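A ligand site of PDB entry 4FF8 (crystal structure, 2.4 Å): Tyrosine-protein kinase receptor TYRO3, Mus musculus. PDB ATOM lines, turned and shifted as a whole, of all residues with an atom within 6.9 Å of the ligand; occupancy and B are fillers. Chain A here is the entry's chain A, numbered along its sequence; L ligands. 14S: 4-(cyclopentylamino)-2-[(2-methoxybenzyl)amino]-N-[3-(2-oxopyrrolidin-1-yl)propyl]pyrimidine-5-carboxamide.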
ATOM      1  N   ALA A  88      23.667  28.404  -1.808  1.00  0.00           N
ATOM      2  CA  ALA A  88      22.552  28.629  -2.728  1.00  0.00           C
ATOM      3  C   ALA A  88      22.850  29.841  -3.608  1.00  0.00           C
ATOM      4  O   ALA A  88      23.294  30.865  -3.097  1.00  0.00           O
ATOM      5  CB  ALA A  88      21.271  28.870  -1.959  1.00  0.00           C
ATOM      6  N   LYS A  89      22.660  29.701  -4.910  1.00  0.00           N
ATOM      7  CA  LYS A  89      22.835  30.823  -5.838  1.00  0.00           C
ATOM      8  C   LYS A  89      21.709  31.825  -5.644  1.00  0.00           C
ATOM      9  O   LYS A  89      20.616  31.477  -5.205  1.00  0.00           O
ATOM     10  CB  LYS A  89      22.790  30.344  -7.299  1.00  0.00           C
ATOM     11  CG  LYS A  89      23.961  29.504  -7.796  1.00  0.00           C
ATOM     12  CD  LYS A  89      23.561  28.740  -9.060  1.00  0.00           C
ATOM     13  CE  LYS A  89      24.493  27.559  -9.350  1.00  0.00           C
ATOM     14  NZ  LYS A  89      23.916  26.613 -10.355  1.00  0.00           N
ATOM     15  N   LEU A 110      15.224  32.490  -6.326  1.00  0.00           N
ATOM     16  CA  LEU A 110      16.104  31.354  -5.945  1.00  0.00           C
ATOM     17  C   LEU A 110      15.939  30.135  -6.892  1.00  0.00           C
ATOM     18  O   LEU A 110      14.871  29.949  -7.478  1.00  0.00           O
ATOM     19  CB  LEU A 110      15.791  30.883  -4.509  1.00  0.00           C
ATOM     20  CG  LEU A 110      16.061  31.819  -3.328  1.00  0.00           C
ATOM     21  CD1 LEU A 110      15.409  31.304  -2.054  1.00  0.00           C
ATOM     22  CD2 LEU A 110      17.558  32.018  -3.105  1.00  0.00           C
ATOM     23  N   PRO A 111      16.975  29.271  -7.001  1.00  0.00           N
ATOM     24  CA  PRO A 111      16.812  28.101  -7.859  1.00  0.00           C
ATOM     25  C   PRO A 111      15.752  27.181  -7.302  1.00  0.00           C
ATOM     26  O   PRO A 111      15.434  27.239  -6.120  1.00  0.00           O
ATOM     27  CB  PRO A 111      18.182  27.417  -7.841  1.00  0.00           C
ATOM     28  CG  PRO A 111      19.120  28.419  -7.258  1.00  0.00           C
ATOM     29  CD  PRO A 111      18.295  29.286  -6.356  1.00  0.00           C
ATOM     30  N   PHE A 112      15.202  26.340  -8.166  1.00  0.00           N
ATOM     31  CA  PHE A 112      14.228  25.345  -7.751  1.00  0.00           C
ATOM     32  C   PHE A 112      15.015  24.100  -7.358  1.00  0.00           C
ATOM     33  O   PHE A 112      15.852  23.667  -8.136  1.00  0.00           O
ATOM     34  CB  PHE A 112      13.255  25.028  -8.868  1.00  0.00           C
ATOM     35  CG  PHE A 112      12.315  23.904  -8.560  1.00  0.00           C
ATOM     36  CD1 PHE A 112      11.184  24.141  -7.803  1.00  0.00           C
ATOM     37  CD2 PHE A 112      12.573  22.625  -9.003  1.00  0.00           C
ATOM     38  CE1 PHE A 112      10.314  23.112  -7.492  1.00  0.00           C
ATOM     39  CE2 PHE A 112      11.708  21.583  -8.710  1.00  0.00           C
ATOM     40  CZ  PHE A 112      10.572  21.827  -7.959  1.00  0.00           C
ATOM     41  N   MET A 113      14.733  23.555  -6.163  1.00  0.00           N
ATOM     42  CA  MET A 113      15.521  22.450  -5.572  1.00  0.00           C
ATOM     43  C   MET A 113      14.644  21.199  -5.471  1.00  0.00           C
ATOM     44  O   MET A 113      13.775  21.110  -4.594  1.00  0.00           O
ATOM     45  CB  MET A 113      16.003  22.853  -4.185  1.00  0.00           C
ATOM     46  CG  MET A 113      16.750  24.172  -4.094  1.00  0.00           C
ATOM     47  SD  MET A 113      18.435  24.129  -4.741  1.00  0.00           S
ATOM     48  CE  MET A 113      19.308  23.077  -3.588  1.00  0.00           C
ATOM     49  N   LYS A 114      14.867  20.218  -6.340  1.00  0.00           N
ATOM     50  CA  LYS A 114      13.916  19.111  -6.523  1.00  0.00           C
ATOM     51  C   LYS A 114      13.611  18.334  -5.222  1.00  0.00           C
ATOM     52  O   LYS A 114      12.504  17.814  -5.047  1.00  0.00           O
ATOM     53  CB  LYS A 114      14.428  18.135  -7.579  1.00  0.00           C
ATOM     54  CG  LYS A 114      13.350  17.296  -8.236  1.00  0.00           C
ATOM     55  CD  LYS A 114      13.967  16.127  -9.017  1.00  0.00           C
ATOM     56  CE  LYS A 114      13.300  15.915 -10.365  1.00  0.00           C
ATOM     57  NZ  LYS A 114      11.817  15.846 -10.306  1.00  0.00           N
ATOM     58  N   HIS A 115      14.578  18.275  -4.331  1.00  0.00           N
ATOM     59  CA  HIS A 115      14.481  17.404  -3.187  1.00  0.00           C
ATOM     60  C   HIS A 115      14.296  18.156  -1.879  1.00  0.00           C
ATOM     61  O   HIS A 115      14.541  17.589  -0.816  1.00  0.00           O
ATOM     62  CB  HIS A 115      15.762  16.579  -3.099  1.00  0.00           C
ATOM     63  CG  HIS A 115      16.029  15.756  -4.325  1.00  0.00           C
ATOM     64  ND1 HIS A 115      15.157  14.789  -4.774  1.00  0.00           N
ATOM     65  CD2 HIS A 115      17.078  15.738  -5.173  1.00  0.00           C
ATOM     66  CE1 HIS A 115      15.654  14.222  -5.853  1.00  0.00           C
ATOM     67  NE2 HIS A 115      16.830  14.772  -6.119  1.00  0.00           N
ATOM     68  N   GLY A 116      13.928  19.429  -1.942  1.00  0.00           N
ATOM     69  CA  GLY A 116      13.515  20.168  -0.760  1.00  0.00           C
ATOM     70  C   GLY A 116      14.599  20.646   0.163  1.00  0.00           C
ATOM     71  O   GLY A 116      15.764  20.609  -0.177  1.00  0.00           O
ATOM     72  N   ASP A 117      14.209  21.154   1.340  1.00  0.00           N
ATOM     73  CA  ASP A 117      15.168  21.417   2.401  1.00  0.00           C
ATOM     74  C   ASP A 117      15.623  20.124   3.073  1.00  0.00           C
ATOM     75  O   ASP A 117      14.965  19.077   2.967  1.00  0.00           O
ATOM     76  CB  ASP A 117      14.602  22.438   3.395  1.00  0.00           C
ATOM     77  CG  ASP A 117      13.614  21.833   4.366  1.00  0.00           C
ATOM     78  OD1 ASP A 117      13.934  20.816   5.015  1.00  0.00           O
ATOM     79  OD2 ASP A 117      12.528  22.429   4.521  1.00  0.00           O
ATOM     80  N   ALA A 120      13.082  18.756   6.143  1.00  0.00           N
ATOM     81  CA  ALA A 120      11.886  18.050   5.618  1.00  0.00           C
ATOM     82  C   ALA A 120      12.300  16.760   4.967  1.00  0.00           C
ATOM     83  O   ALA A 120      11.666  15.732   5.184  1.00  0.00           O
ATOM     84  CB  ALA A 120      11.105  18.912   4.633  1.00  0.00           C
ATOM     85  N   PHE A 121      13.401  16.814   4.239  1.00  0.00           N
ATOM     86  CA  PHE A 121      13.945  15.621   3.639  1.00  0.00           C
ATOM     87  C   PHE A 121      14.227  14.578   4.715  1.00  0.00           C
ATOM     88  O   PHE A 121      13.560  13.555   4.741  1.00  0.00           O
ATOM     89  CB  PHE A 121      15.202  15.892   2.824  1.00  0.00           C
ATOM     90  CG  PHE A 121      15.787  14.653   2.195  1.00  0.00           C
ATOM     91  CD1 PHE A 121      16.718  13.895   2.878  1.00  0.00           C
ATOM     92  CD2 PHE A 121      15.344  14.206   0.966  1.00  0.00           C
ATOM     93  CE1 PHE A 121      17.230  12.735   2.320  1.00  0.00           C
ATOM     94  CE2 PHE A 121      15.839  13.050   0.407  1.00  0.00           C
ATOM     95  CZ  PHE A 121      16.774  12.306   1.087  1.00  0.00           C
ATOM     96  N   LEU A 122      15.204  14.834   5.591  1.00  0.00           N
ATOM     97  CA  LEU A 122      15.583  13.840   6.631  1.00  0.00           C
ATOM     98  C   LEU A 122      14.362  13.338   7.383  1.00  0.00           C
ATOM     99  O   LEU A 122      14.376  12.213   7.856  1.00  0.00           O
ATOM    100  CB  LEU A 122      16.581  14.398   7.653  1.00  0.00           C
ATOM    101  CG  LEU A 122      18.035  14.609   7.213  1.00  0.00           C
ATOM    102  CD1 LEU A 122      18.594  15.749   8.026  1.00  0.00           C
ATOM    103  CD2 LEU A 122      18.887  13.367   7.386  1.00  0.00           C
ATOM    104  N   ALA A 124      11.191  13.139   5.949  1.00  0.00           N
ATOM    105  CA  ALA A 124      10.515  12.215   5.030  1.00  0.00           C
ATOM    106  C   ALA A 124      11.045  10.797   5.206  1.00  0.00           C
ATOM    107  O   ALA A 124      10.274   9.840   5.241  1.00  0.00           O
ATOM    108  CB  ALA A 124      10.687  12.670   3.595  1.00  0.00           C
ATOM    109  N   ARG A 166      16.689  23.000   8.297  1.00  0.00           N
ATOM    110  CA  ARG A 166      15.607  23.616   7.537  1.00  0.00           C
ATOM    111  C   ARG A 166      16.154  24.559   6.471  1.00  0.00           C
ATOM    112  O   ARG A 166      15.618  24.633   5.367  1.00  0.00           O
ATOM    113  CB  ARG A 166      14.594  24.324   8.449  1.00  0.00           C
ATOM    114  CG  ARG A 166      15.125  25.495   9.267  1.00  0.00           C
ATOM    115  CD  ARG A 166      14.045  26.272  10.067  1.00  0.00           C
ATOM    116  NE  ARG A 166      14.645  27.273  10.973  1.00  0.00           N
ATOM    117  CZ  ARG A 166      15.320  26.957  12.089  1.00  0.00           C
ATOM    118  NH1 ARG A 166      15.482  25.683  12.461  1.00  0.00           N
ATOM    119  NH2 ARG A 166      15.903  27.914  12.836  1.00  0.00           N
ATOM    120  N   ASN A 167      17.255  25.244   6.778  1.00  0.00           N
ATOM    121  CA  ASN A 167      17.779  26.254   5.855  1.00  0.00           C
ATOM    122  C   ASN A 167      18.961  25.773   5.026  1.00  0.00           C
ATOM    123  O   ASN A 167      19.797  26.579   4.604  1.00  0.00           O
ATOM    124  CB  ASN A 167      18.165  27.508   6.642  1.00  0.00           C
ATOM    125  CG  ASN A 167      16.953  28.232   7.209  1.00  0.00           C
ATOM    126  OD1 ASN A 167      15.869  28.186   6.633  1.00  0.00           O
ATOM    127  ND2 ASN A 167      17.145  28.926   8.319  1.00  0.00           N
ATOM    128  N   CYS A 168      19.080  24.473   4.844  1.00  0.00           N
ATOM    129  CA  CYS A 168      20.030  23.915   3.899  1.00  0.00           C
ATOM    130  C   CYS A 168      19.194  23.220   2.849  1.00  0.00           C
ATOM    131  O   CYS A 168      18.137  22.697   3.174  1.00  0.00           O
ATOM    132  CB  CYS A 168      20.961  22.925   4.572  1.00  0.00           C
ATOM    133  SG  CYS A 168      22.093  23.667   5.748  1.00  0.00           S
ATOM    134  N   MET A 169      19.658  23.222   1.598  1.00  0.00           N
ATOM    135  CA  MET A 169      18.831  22.726   0.512  1.00  0.00           C
ATOM    136  C   MET A 169      19.541  21.604  -0.254  1.00  0.00           C
ATOM    137  O   MET A 169      20.721  21.684  -0.481  1.00  0.00           O
ATOM    138  CB  MET A 169      18.416  23.869  -0.430  1.00  0.00           C
ATOM    139  CG  MET A 169      17.518  24.931   0.182  1.00  0.00           C
ATOM    140  SD  MET A 169      15.853  24.386   0.687  1.00  0.00           S
ATOM    141  CE  MET A 169      14.908  24.760  -0.795  1.00  0.00           C
ATOM    142  N   LEU A 170      18.798  20.550  -0.602  1.00  0.00           N
ATOM    143  CA  LEU A 170      19.275  19.479  -1.484  1.00  0.00           C
ATOM    144  C   LEU A 170      18.916  19.711  -2.958  1.00  0.00           C
ATOM    145  O   LEU A 170      17.736  19.730  -3.315  1.00  0.00           O
ATOM    146  CB  LEU A 170      18.594  18.169  -1.104  1.00  0.00           C
ATOM    147  CG  LEU A 170      18.939  17.526   0.207  1.00  0.00           C
ATOM    148  CD1 LEU A 170      17.931  16.408   0.497  1.00  0.00           C
ATOM    149  CD2 LEU A 170      20.390  17.042   0.180  1.00  0.00           C
ATOM    150  N   CYS A 177      23.289  22.589  -0.310  1.00  0.00           N
ATOM    151  CA  CYS A 177      23.797  23.966  -0.303  1.00  0.00           C
ATOM    152  C   CYS A 177      23.148  24.766   0.812  1.00  0.00           C
ATOM    153  O   CYS A 177      22.009  24.499   1.193  1.00  0.00           O
ATOM    154  CB  CYS A 177      23.599  24.643  -1.631  1.00  0.00           C
ATOM    155  SG  CYS A 177      21.892  25.070  -1.964  1.00  0.00           S
ATOM    156  N   VAL A 178      23.918  25.721   1.360  1.00  0.00           N
ATOM    157  CA  VAL A 178      23.474  26.528   2.475  1.00  0.00           C
ATOM    158  C   VAL A 178      22.703  27.720   1.927  1.00  0.00           C
ATOM    159  O   VAL A 178      23.195  28.412   1.045  1.00  0.00           O
ATOM    160  CB  VAL A 178      24.665  27.061   3.298  1.00  0.00           C
ATOM    161  CG1 VAL A 178      24.188  28.018   4.378  1.00  0.00           C
ATOM    162  CG2 VAL A 178      25.469  25.931   3.900  1.00  0.00           C
ATOM    163  N   ALA A 179      21.517  27.963   2.475  1.00  0.00           N
ATOM    164  CA  ALA A 179      20.619  29.050   2.045  1.00  0.00           C
ATOM    165  C   ALA A 179      20.334  30.035   3.174  1.00  0.00           C
ATOM    166  O   ALA A 179      19.177  30.409   3.392  1.00  0.00           O
ATOM    167  CB  ALA A 179      19.312  28.478   1.564  1.00  0.00           C
HETATM  168  O33 14S L   1      11.042  15.905  -2.513  1.00  0.00           O
HETATM  169  C28 14S L   1      10.851  16.190  -1.339  1.00  0.00           C
HETATM  170  C32 14S L   1      11.324  15.337  -0.187  1.00  0.00           C
HETATM  171  C34 14S L   1      10.761  16.074   1.051  1.00  0.00           C
HETATM  172  C29 14S L   1      10.221  17.446   0.575  1.00  0.00           C
HETATM  173  N24 14S L   1      10.222  17.272  -0.869  1.00  0.00           N
HETATM  174  C21 14S L   1       9.516  18.270  -1.688  1.00  0.00           C
HETATM  175  C19 14S L   1      10.595  19.246  -2.173  1.00  0.00           C
HETATM  176  C15 14S L   1      10.158  20.010  -3.420  1.00  0.00           C
HETATM  177  N10 14S L   1      10.883  21.252  -3.572  1.00  0.00           N
HETATM  178  C6  14S L   1      10.585  22.362  -2.887  1.00  0.00           C
HETATM  179  O11 14S L   1       9.680  22.395  -2.077  1.00  0.00           O
HETATM  180  C2  14S L   1      11.407  23.599  -3.122  1.00  0.00           C
HETATM  181  C1  14S L   1      11.540  24.591  -2.158  1.00  0.00           C
HETATM  182  N4  14S L   1      10.911  24.470  -0.964  1.00  0.00           N
HETATM  183  C8  14S L   1      10.967  25.461   0.114  1.00  0.00           C
HETATM  184  C14 14S L   1      12.223  25.299   0.972  1.00  0.00           C
HETATM  185  C18 14S L   1      11.816  24.834   2.356  1.00  0.00           C
HETATM  186  C17 14S L   1      10.306  24.650   2.360  1.00  0.00           C
HETATM  187  C13 14S L   1       9.782  25.242   1.047  1.00  0.00           C
HETATM  188  C5  14S L   1      12.069  23.752  -4.330  1.00  0.00           C
HETATM  189  N9  14S L   1      12.807  24.841  -4.556  1.00  0.00           N
HETATM  190  C7  14S L   1      12.933  25.812  -3.630  1.00  0.00           C
HETATM  191  N3  14S L   1      12.314  25.681  -2.437  1.00  0.00           N
HETATM  192  N12 14S L   1      13.709  26.876  -3.924  1.00  0.00           N
HETATM  193  C16 14S L   1      13.864  27.958  -2.967  1.00  0.00           C
HETATM  194  C20 14S L   1      15.284  28.093  -2.440  1.00  0.00           C
HETATM  195  C23 14S L   1      16.362  27.672  -3.217  1.00  0.00           C
HETATM  196  C27 14S L   1      17.661  27.806  -2.733  1.00  0.00           C
HETATM  197  C30 14S L   1      17.869  28.358  -1.469  1.00  0.00           C
HETATM  198  C25 14S L   1      16.797  28.776  -0.700  1.00  0.00           C
HETATM  199  C22 14S L   1      15.488  28.631  -1.173  1.00  0.00           C
HETATM  200  O26 14S L   1      14.425  29.059  -0.414  1.00  0.00           O
HETATM  201  C31 14S L   1      14.168  28.505   0.872  1.00  0.00           C
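The backbone carbonyl oxygen (O) of Met 113 sits at hydrogen-bond distance from a nitrogen (N10) of the ligand, 3.1 Å away. The backbone NH (N) of Met 113 is in hydrogen-bond range of a nitrogen (N9) of the ligand, 2.8 Å away. The backbone carbonyl oxygen of Pro 111 sits at hydrogen-bond distance from a nitrogen (N12) of the ligand.
SD of Met 169 lies close to N of Asp 117. O of Asn 167 is in hydrogen-bond range of N of Ala 179 (3.1 Å). N of Met 169 lies within hydrogen-bond range of O of Cys 177. The backbone NH of Ala 88 lies close to the side-chain sulfur of Cys 177 (3.8 Å). The backbone NH (N) of Ala 120 lies within hydrogen-bond range of the side-chain carboxylate (OD1) of Asp 117. O of Val 178 is in hydrogen-bond range of N of Ala 88. N of Leu 170 is in hydrogen-bond range of O of Gly 116 (3.1 Å).
The backbone carbonyl oxygen of Lys 114 lies close to an oxygen (O33) of the ligand, at 3.5 Å. Ala 88 touches the ligand. Leu 110 touches the ligand. CA of Phe 112 touches N9 of the ligand, 3.5 Å away. His 115 touches the ligand. N of Gly 116 touches C19 of the ligand, at 3.3 Å. OD2 of Asp 117 touches C18 of the ligand, 3.3 Å away. CE of Met 169 touches N3 of the ligand, 3.2 Å away. CB of Ala 179 touches C30 of the ligand, at 3.4 Å. Hydrophobic or aromatic side chains that line the ligand: Ala 88, Leu 110, Pro 111, Phe 112, Met 113, Met 169 and Ala 179.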
